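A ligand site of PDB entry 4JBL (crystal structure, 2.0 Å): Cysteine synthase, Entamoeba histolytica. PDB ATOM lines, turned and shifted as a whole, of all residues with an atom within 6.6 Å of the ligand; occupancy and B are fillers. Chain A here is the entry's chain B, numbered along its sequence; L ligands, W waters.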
ATOM      1  N   SER A  56      -3.190  10.120 -17.156  1.00  0.00           N
ATOM      2  CA  SER A  56      -4.011  10.980 -16.385  1.00  0.00           C
ATOM      3  C   SER A  56      -4.831  10.252 -15.378  1.00  0.00           C
ATOM      4  O   SER A  56      -4.960   9.002 -15.405  1.00  0.00           O
ATOM      5  CB  SER A  56      -4.892  11.801 -17.366  1.00  0.00           C
ATOM      6  OG  SER A  56      -6.139  11.232 -17.543  1.00  0.00           O
ATOM      7  N1  LLP A  58      -7.602  17.913 -14.438  1.00  0.00           N
ATOM      8  C2  LLP A  58      -7.543  17.171 -15.569  1.00  0.00           C
ATOM      9  C2' LLP A  58      -6.451  17.498 -16.607  1.00  0.00           C
ATOM     10  C3  LLP A  58      -8.580  16.137 -15.770  1.00  0.00           C
ATOM     11  O3  LLP A  58      -8.654  15.389 -16.831  1.00  0.00           O
ATOM     12  C4  LLP A  58      -9.567  15.921 -14.699  1.00  0.00           C
ATOM     13  C4' LLP A  58     -10.693  14.922 -14.749  1.00  0.00           C
ATOM     14  C5  LLP A  58      -9.504  16.829 -13.551  1.00  0.00           C
ATOM     15  C6  LLP A  58      -8.483  17.765 -13.454  1.00  0.00           C
ATOM     16  C5' LLP A  58     -10.541  16.730 -12.452  1.00  0.00           C
ATOM     17  OP4 LLP A  58     -10.774  15.394 -11.953  1.00  0.00           O
ATOM     18  P   LLP A  58     -12.294  15.007 -11.512  1.00  0.00           P
ATOM     19  OP1 LLP A  58     -12.083  13.707 -10.745  1.00  0.00           O
ATOM     20  OP2 LLP A  58     -13.011  14.846 -12.794  1.00  0.00           O
ATOM     21  OP3 LLP A  58     -12.923  16.132 -10.701  1.00  0.00           O
ATOM     22  N   LLP A  58      -7.854  10.008 -15.318  1.00  0.00           N
ATOM     23  CA  LLP A  58      -9.109   9.433 -15.885  1.00  0.00           C
ATOM     24  CB  LLP A  58      -9.495  10.164 -17.147  1.00  0.00           C
ATOM     25  CG  LLP A  58      -9.945  11.625 -16.834  1.00  0.00           C
ATOM     26  CD  LLP A  58     -11.117  11.691 -15.808  1.00  0.00           C
ATOM     27  CE  LLP A  58     -11.791  13.057 -15.815  1.00  0.00           C
ATOM     28  NZ  LLP A  58     -10.826  14.168 -15.906  1.00  0.00           N
ATOM     29  C   LLP A  58      -8.892   7.994 -16.214  1.00  0.00           C
ATOM     30  O   LLP A  58      -9.829   7.249 -16.412  1.00  0.00           O
ATOM     31  N   GLU A  83     -19.365   8.605 -25.268  1.00  0.00           N
ATOM     32  CA  GLU A  83     -19.190   9.611 -24.244  1.00  0.00           C
ATOM     33  C   GLU A  83     -18.839  11.053 -24.708  1.00  0.00           C
ATOM     34  O   GLU A  83     -18.419  11.228 -25.809  1.00  0.00           O
ATOM     35  CB  GLU A  83     -18.102   9.198 -23.285  1.00  0.00           C
ATOM     36  CG  GLU A  83     -17.889  10.203 -22.200  1.00  0.00           C
ATOM     37  CD  GLU A  83     -19.036  10.253 -21.238  1.00  0.00           C
ATOM     38  OE1 GLU A  83     -20.131   9.881 -21.620  1.00  0.00           O
ATOM     39  OE2 GLU A  83     -18.810  10.562 -20.093  1.00  0.00           O
ATOM     40  N   SER A  84     -18.810  12.071 -23.823  1.00  0.00           N
ATOM     41  CA  SER A  84     -18.346  13.479 -23.938  1.00  0.00           C
ATOM     42  C   SER A  84     -17.390  13.856 -22.836  1.00  0.00           C
ATOM     43  O   SER A  84     -17.705  13.725 -21.589  1.00  0.00           O
ATOM     44  CB  SER A  84     -19.538  14.443 -23.921  1.00  0.00           C
ATOM     45  OG  SER A  84     -20.231  14.371 -22.693  1.00  0.00           O
ATOM     46  N   THR A  85     -16.423  14.403 -23.424  1.00  0.00           N
ATOM     47  CA  THR A  85     -15.304  14.627 -22.508  1.00  0.00           C
ATOM     48  C   THR A  85     -14.550  15.983 -22.674  1.00  0.00           C
ATOM     49  O   THR A  85     -14.626  16.625 -23.756  1.00  0.00           O
ATOM     50  CB  THR A  85     -14.400  13.355 -22.543  1.00  0.00           C
ATOM     51  OG1 THR A  85     -13.062  13.689 -22.276  1.00  0.00           O
ATOM     52  CG2 THR A  85     -14.453  12.660 -23.860  1.00  0.00           C
ATOM     53  N   SER A  86     -13.723  16.370 -21.725  1.00  0.00           N
ATOM     54  CA  SER A  86     -12.748  17.387 -22.069  1.00  0.00           C
ATOM     55  C   SER A  86     -11.412  16.804 -22.594  1.00  0.00           C
ATOM     56  O   SER A  86     -10.474  17.535 -22.876  1.00  0.00           O
ATOM     57  CB  SER A  86     -12.496  18.349 -20.937  1.00  0.00           C
ATOM     58  OG  SER A  86     -11.711  17.763 -19.945  1.00  0.00           O
ATOM     59  N   GLY A  87     -11.345  15.502 -22.707  1.00  0.00           N
ATOM     60  CA  GLY A  87     -10.213  14.877 -23.313  1.00  0.00           C
ATOM     61  C   GLY A  87      -9.734  13.634 -22.636  1.00  0.00           C
ATOM     62  O   GLY A  87      -9.745  12.595 -23.236  1.00  0.00           O
ATOM     63  N   ASN A  88      -9.307  13.753 -21.409  1.00  0.00           N
ATOM     64  CA  ASN A  88      -8.712  12.641 -20.723  1.00  0.00           C
ATOM     65  C   ASN A  88      -9.665  11.481 -20.572  1.00  0.00           C
ATOM     66  O   ASN A  88      -9.313  10.401 -20.784  1.00  0.00           O
ATOM     67  CB  ASN A  88      -8.127  13.070 -19.412  1.00  0.00           C
ATOM     68  CG  ASN A  88      -6.843  13.873 -19.569  1.00  0.00           C
ATOM     69  OD1 ASN A  88      -6.557  14.698 -18.764  1.00  0.00           O
ATOM     70  ND2 ASN A  88      -6.135  13.660 -20.606  1.00  0.00           N
ATOM     71  N   THR A  89     -10.895  11.738 -20.227  1.00  0.00           N
ATOM     72  CA  THR A  89     -11.887  10.626 -20.165  1.00  0.00           C
ATOM     73  C   THR A  89     -12.017   9.845 -21.487  1.00  0.00           C
ATOM     74  O   THR A  89     -12.092   8.591 -21.469  1.00  0.00           O
ATOM     75  CB  THR A  89     -13.279  11.042 -19.620  1.00  0.00           C
ATOM     76  OG1 THR A  89     -13.165  11.612 -18.313  1.00  0.00           O
ATOM     77  CG2 THR A  89     -14.271   9.839 -19.472  1.00  0.00           C
ATOM     78  N   GLY A  90     -12.047  10.528 -22.643  1.00  0.00           N
ATOM     79  CA  GLY A  90     -12.178   9.783 -23.911  1.00  0.00           C
ATOM     80  C   GLY A  90     -10.954   8.865 -24.111  1.00  0.00           C
ATOM     81  O   GLY A  90     -11.051   7.713 -24.597  1.00  0.00           O
ATOM     82  N   MET A 112     -10.289  22.371 -26.480  1.00  0.00           N
ATOM     83  CA  MET A 112      -9.370  21.517 -25.725  1.00  0.00           C
ATOM     84  C   MET A 112      -8.105  21.206 -26.525  1.00  0.00           C
ATOM     85  O   MET A 112      -8.182  21.132 -27.739  1.00  0.00           O
ATOM     86  CB  MET A 112     -10.022  20.186 -25.327  1.00  0.00           C
ATOM     87  CG  MET A 112     -11.213  20.231 -24.392  1.00  0.00           C
ATOM     88  SD  MET A 112     -11.189  21.524 -23.185  1.00  0.00           S
ATOM     89  CE  MET A 112     -10.945  20.695 -21.675  1.00  0.00           C
ATOM     90  N   ARG A 116      -4.934  16.034 -27.119  1.00  0.00           N
ATOM     91  CA  ARG A 116      -6.054  15.135 -26.728  1.00  0.00           C
ATOM     92  C   ARG A 116      -6.712  14.536 -27.962  1.00  0.00           C
ATOM     93  O   ARG A 116      -7.005  13.356 -27.990  1.00  0.00           O
ATOM     94  CB  ARG A 116      -7.085  15.902 -25.893  1.00  0.00           C
ATOM     95  CG  ARG A 116      -6.561  16.364 -24.541  1.00  0.00           C
ATOM     96  CD  ARG A 116      -7.222  17.676 -24.132  1.00  0.00           C
ATOM     97  NE  ARG A 116      -7.319  17.775 -22.662  1.00  0.00           N
ATOM     98  CZ  ARG A 116      -6.320  18.027 -21.799  1.00  0.00           C
ATOM     99  NH1 ARG A 116      -5.092  18.283 -22.235  1.00  0.00           N
ATOM    100  NH2 ARG A 116      -6.551  18.088 -20.461  1.00  0.00           N
ATOM    101  N   MET A 136     -18.491  22.048 -22.003  1.00  0.00           N
ATOM    102  CA  MET A 136     -18.841  20.690 -21.667  1.00  0.00           C
ATOM    103  C   MET A 136     -20.350  20.419 -21.901  1.00  0.00           C
ATOM    104  O   MET A 136     -20.699  19.391 -22.431  1.00  0.00           O
ATOM    105  CB  MET A 136     -18.370  20.383 -20.244  1.00  0.00           C
ATOM    106  CG  MET A 136     -16.857  20.112 -20.086  1.00  0.00           C
ATOM    107  SD  MET A 136     -16.063  19.064 -21.330  1.00  0.00           S
ATOM    108  CE  MET A 136     -16.965  17.540 -21.209  1.00  0.00           C
ATOM    109  N   GLN A 159     -19.913  10.382 -17.446  1.00  0.00           N
ATOM    110  CA  GLN A 159     -18.866  10.506 -16.377  1.00  0.00           C
ATOM    111  C   GLN A 159     -19.288  11.502 -15.287  1.00  0.00           C
ATOM    112  O   GLN A 159     -18.788  11.438 -14.162  1.00  0.00           O
ATOM    113  CB  GLN A 159     -17.569  10.968 -16.996  1.00  0.00           C
ATOM    114  CG  GLN A 159     -17.662  12.346 -17.685  1.00  0.00           C
ATOM    115  CD  GLN A 159     -16.292  12.874 -18.088  1.00  0.00           C
ATOM    116  OE1 GLN A 159     -15.272  12.615 -17.400  1.00  0.00           O
ATOM    117  NE2 GLN A 159     -16.240  13.550 -19.182  1.00  0.00           N
ATOM    118  N   PHE A 160     -20.187  12.447 -15.613  1.00  0.00           N
ATOM    119  CA  PHE A 160     -20.642  13.394 -14.585  1.00  0.00           C
ATOM    120  C   PHE A 160     -21.732  12.862 -13.690  1.00  0.00           C
ATOM    121  O   PHE A 160     -22.068  13.526 -12.708  1.00  0.00           O
ATOM    122  CB  PHE A 160     -21.133  14.670 -15.254  1.00  0.00           C
ATOM    123  CG  PHE A 160     -20.037  15.408 -15.999  1.00  0.00           C
ATOM    124  CD1 PHE A 160     -19.202  16.263 -15.313  1.00  0.00           C
ATOM    125  CD2 PHE A 160     -19.875  15.218 -17.348  1.00  0.00           C
ATOM    126  CE1 PHE A 160     -18.177  16.940 -15.975  1.00  0.00           C
ATOM    127  CE2 PHE A 160     -18.858  15.873 -18.016  1.00  0.00           C
ATOM    128  CZ  PHE A 160     -18.039  16.746 -17.329  1.00  0.00           C
ATOM    129  N   VAL A 191     -11.512  20.444  -9.383  1.00  0.00           N
ATOM    130  CA  VAL A 191     -12.766  19.688  -9.695  1.00  0.00           C
ATOM    131  C   VAL A 191     -13.238  19.781 -11.149  1.00  0.00           C
ATOM    132  O   VAL A 191     -13.517  20.853 -11.623  1.00  0.00           O
ATOM    133  CB  VAL A 191     -13.942  20.171  -8.794  1.00  0.00           C
ATOM    134  CG1 VAL A 191     -15.242  19.480  -9.217  1.00  0.00           C
ATOM    135  CG2 VAL A 191     -13.635  19.964  -7.330  1.00  0.00           C
ATOM    136  N   GLY A 192     -13.379  18.633 -11.828  1.00  0.00           N
ATOM    137  CA  GLY A 192     -13.942  18.561 -13.162  1.00  0.00           C
ATOM    138  C   GLY A 192     -15.248  17.825 -13.111  1.00  0.00           C
ATOM    139  O   GLY A 192     -16.355  18.457 -12.939  1.00  0.00           O
ATOM    140  N   THR A 193     -15.160  16.485 -13.077  1.00  0.00           N
ATOM    141  CA  THR A 193     -16.354  15.697 -12.800  1.00  0.00           C
ATOM    142  C   THR A 193     -16.740  15.674 -11.327  1.00  0.00           C
ATOM    143  O   THR A 193     -17.882  15.357 -11.023  1.00  0.00           O
ATOM    144  CB  THR A 193     -16.241  14.231 -13.290  1.00  0.00           C
ATOM    145  OG1 THR A 193     -15.269  13.512 -12.495  1.00  0.00           O
ATOM    146  CG2 THR A 193     -15.883  14.167 -14.801  1.00  0.00           C
ATOM    147  N   HIS A 232     -12.905  30.254 -19.210  1.00  0.00           N
ATOM    148  CA  HIS A 232     -11.728  30.222 -18.364  1.00  0.00           C
ATOM    149  C   HIS A 232     -10.781  29.415 -19.132  1.00  0.00           C
ATOM    150  O   HIS A 232     -11.173  28.841 -20.109  1.00  0.00           O
ATOM    151  CB  HIS A 232     -12.026  29.589 -16.986  1.00  0.00           C
ATOM    152  CG  HIS A 232     -12.356  28.115 -17.048  1.00  0.00           C
ATOM    153  ND1 HIS A 232     -11.395  27.126 -17.053  1.00  0.00           N
ATOM    154  CD2 HIS A 232     -13.573  27.465 -17.222  1.00  0.00           C
ATOM    155  CE1 HIS A 232     -11.980  25.929 -17.162  1.00  0.00           C
ATOM    156  NE2 HIS A 232     -13.319  26.116 -17.260  1.00  0.00           N
ATOM    157  N   ILE A 234      -8.535  26.921 -17.460  1.00  0.00           N
ATOM    158  CA  ILE A 234      -7.917  25.796 -16.753  1.00  0.00           C
ATOM    159  C   ILE A 234      -8.440  24.493 -17.328  1.00  0.00           C
ATOM    160  O   ILE A 234      -9.424  23.918 -16.873  1.00  0.00           O
ATOM    161  CB  ILE A 234      -8.014  25.873 -15.227  1.00  0.00           C
ATOM    162  CG1 ILE A 234      -7.644  27.288 -14.733  1.00  0.00           C
ATOM    163  CG2 ILE A 234      -7.030  24.860 -14.552  1.00  0.00           C
ATOM    164  CD1 ILE A 234      -8.020  27.492 -13.266  1.00  0.00           C
ATOM    165  N   GLN A 235      -7.793  24.046 -18.393  1.00  0.00           N
ATOM    166  CA  GLN A 235      -8.224  22.806 -19.029  1.00  0.00           C
ATOM    167  C   GLN A 235      -8.319  21.597 -18.090  1.00  0.00           C
ATOM    168  O   GLN A 235      -7.444  21.379 -17.267  1.00  0.00           O
ATOM    169  CB  GLN A 235      -7.320  22.466 -20.189  1.00  0.00           C
ATOM    170  CG  GLN A 235      -7.678  23.237 -21.439  1.00  0.00           C
ATOM    171  CD  GLN A 235      -6.851  22.790 -22.673  1.00  0.00           C
ATOM    172  OE1 GLN A 235      -6.713  21.595 -22.980  1.00  0.00           O
ATOM    173  NE2 GLN A 235      -6.294  23.772 -23.363  1.00  0.00           N
ATOM    174  N   GLY A 236      -9.429  20.913 -18.184  1.00  0.00           N
ATOM    175  CA  GLY A 236      -9.722  19.746 -17.416  1.00  0.00           C
ATOM    176  C   GLY A 236     -10.635  19.922 -16.240  1.00  0.00           C
ATOM    177  O   GLY A 236     -11.048  18.952 -15.699  1.00  0.00           O
ATOM    178  N   ILE A 237     -10.879  21.188 -15.850  1.00  0.00           N
ATOM    179  CA  ILE A 237     -11.792  21.569 -14.793  1.00  0.00           C
ATOM    180  C   ILE A 237     -12.847  22.645 -15.184  1.00  0.00           C
ATOM    181  O   ILE A 237     -12.975  22.971 -16.313  1.00  0.00           O
ATOM    182  CB  ILE A 237     -11.063  21.921 -13.463  1.00  0.00           C
ATOM    183  CG1 ILE A 237     -10.330  23.242 -13.567  1.00  0.00           C
ATOM    184  CG2 ILE A 237     -10.136  20.800 -13.032  1.00  0.00           C
ATOM    185  CD1 ILE A 237      -9.804  23.749 -12.272  1.00  0.00           C
ATOM    186  N   GLY A 238     -13.565  23.193 -14.222  1.00  0.00           N
ATOM    187  CA  GLY A 238     -14.612  24.175 -14.657  1.00  0.00           C
ATOM    188  C   GLY A 238     -15.569  23.667 -15.711  1.00  0.00           C
ATOM    189  O   GLY A 238     -15.627  24.225 -16.835  1.00  0.00           O
ATOM    190  N   ALA A 239     -16.351  22.644 -15.356  1.00  0.00           N
ATOM    191  CA  ALA A 239     -17.344  22.045 -16.277  1.00  0.00           C
ATOM    192  C   ALA A 239     -18.455  23.035 -16.653  1.00  0.00           C
ATOM    193  O   ALA A 239     -19.044  22.873 -17.685  1.00  0.00           O
ATOM    194  CB  ALA A 239     -17.994  20.850 -15.600  1.00  0.00           C
ATOM    195  N   GLY A 240     -18.709  24.023 -15.789  1.00  0.00           N
ATOM    196  CA  GLY A 240     -19.756  24.996 -16.060  1.00  0.00           C
ATOM    197  C   GLY A 240     -21.084  24.635 -15.429  1.00  0.00           C
ATOM    198  O   GLY A 240     -22.010  25.326 -15.690  1.00  0.00           O
ATOM    199  N   PHE A 241     -21.173  23.545 -14.610  1.00  0.00           N
ATOM    200  CA  PHE A 241     -22.403  23.089 -13.889  1.00  0.00           C
ATOM    201  C   PHE A 241     -21.928  22.285 -12.707  1.00  0.00           C
ATOM    202  O   PHE A 241     -20.712  21.972 -12.611  1.00  0.00           O
ATOM    203  CB  PHE A 241     -23.353  22.215 -14.755  1.00  0.00           C
ATOM    204  CG  PHE A 241     -22.657  21.038 -15.408  1.00  0.00           C
ATOM    205  CD1 PHE A 241     -22.698  19.778 -14.818  1.00  0.00           C
ATOM    206  CD2 PHE A 241     -21.972  21.204 -16.591  1.00  0.00           C
ATOM    207  CE1 PHE A 241     -22.029  18.711 -15.409  1.00  0.00           C
ATOM    208  CE2 PHE A 241     -21.330  20.140 -17.199  1.00  0.00           C
ATOM    209  CZ  PHE A 241     -21.351  18.882 -16.587  1.00  0.00           C
HETATM  210  N1  LIG L   1     -11.671  16.528 -17.513  1.00  0.00           N
HETATM  211  C1  LIG L   1     -12.947  15.727 -17.789  1.00  0.00           C
HETATM  212  C2  LIG L   1     -12.751  14.786 -18.971  1.00  0.00           C
HETATM  213  O1  LIG L   1     -13.650  14.501 -19.760  1.00  0.00           O
HETATM  214  C3  LIG L   1     -14.079  16.691 -17.952  1.00  0.00           C
HETATM  215  C4  LIG L   1     -14.136  17.544 -16.676  1.00  0.00           C
HETATM  216  S1  LIG L   1     -15.153  19.025 -16.888  1.00  0.00           S
HETATM  217  C5  LIG L   1     -14.087  20.159 -17.856  1.00  0.00           C
HETATM  218  O2  LIG L   1     -11.639  14.282 -19.167  1.00  0.00           O
HETATM  219  O   HOH W   1      -9.090  16.558 -19.712  1.00  0.00           O
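Gly 87 touches the ligand. Met 136 touches the ligand (CG to C5, 3.6 Å). Phe 160 touches the ligand. Gly 192 touches the ligand. Thr 193 touches the ligand (N to C4, 3.9 Å). O of Ile 237 touches C5 of the ligand, at 3.4 Å. Ala 239 touches the ligand. Hydrophobic or aromatic side chains that line the ligand: Met 136, Phe 160 and Ala 239. Within 4 Å of the ligand: LLP 58, Thr 85, Ser 86, Gly 87, Asn 88, Thr 89, Met 136, Gln 159, Phe 160, Gly 192, Thr 193, Gly 236, Ile 237 and Ala 239. Along chain A the residues within 4 Å of the ligand span positions 58 to 239.
OG1 of Thr 85 lies within hydrogen-bond range of N of Gly 87 (2.5 Å). The backbone NH (N) of Ser 86 sits close to the side-chain sulfur (SD) of Met 136, 3.6 Å away. NE of Arg 116 sits at hydrogen-bond distance from O of Ser 86 (3.2 Å). NE2 of Gln 159 is in hydrogen-bond range of O of Ser 84, at 2.8 Å. The backbone NH (N) of Gln 159 is in hydrogen-bond range of the side-chain carboxylate (OE2) of Glu 83 (2.9 Å). The side-chain amide oxygen (OD1) of Asn 88 lies within hydrogen-bond range of O3 of LLP 58 (2.9 Å). OP3 of LLP 58 is in hydrogen-bond range of the backbone NH of Gly 192. OP2 of LLP 58 lies within hydrogen-bond range of OG1 of Thr 193 (2.6 Å).
Water W1 lies within hydrogen-bond range of OG of Ser 86, NH2 of Arg 116, O3 of LLP 58, OD1 of Asn 88 and N1 of the ligand.
The side-chain hydroxyl (OG1) of Thr 85 lies within hydrogen-bond range of an oxygen (O1) of the ligand. O1 of the ligand lies within hydrogen-bond range of N of Ser 86 (2.7 Å). The side-chain hydroxyl (OG) of Ser 86 lies within hydrogen-bond range of a nitrogen (N1) of the ligand. NE2 of Gln 159 lies within hydrogen-bond range of O1 of the ligand, 2.8 Å away. The backbone NH of Thr 89 lies within hydrogen-bond range of an oxygen (O2) of the ligand (2.9 Å). O2 of the ligand sits at hydrogen-bond distance from OG1 of Thr 89, 3.2 Å away. NZ of LLP 58 is in hydrogen-bond range of a nitrogen (N1) of the ligand. A nitrogen (N1) of the ligand sits at hydrogen-bond distance from the backbone carbonyl oxygen (O) of Gly 236. The backbone NH (N) of Asn 88 sits at hydrogen-bond distance from an oxygen (O2) of the ligand (3.3 Å).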
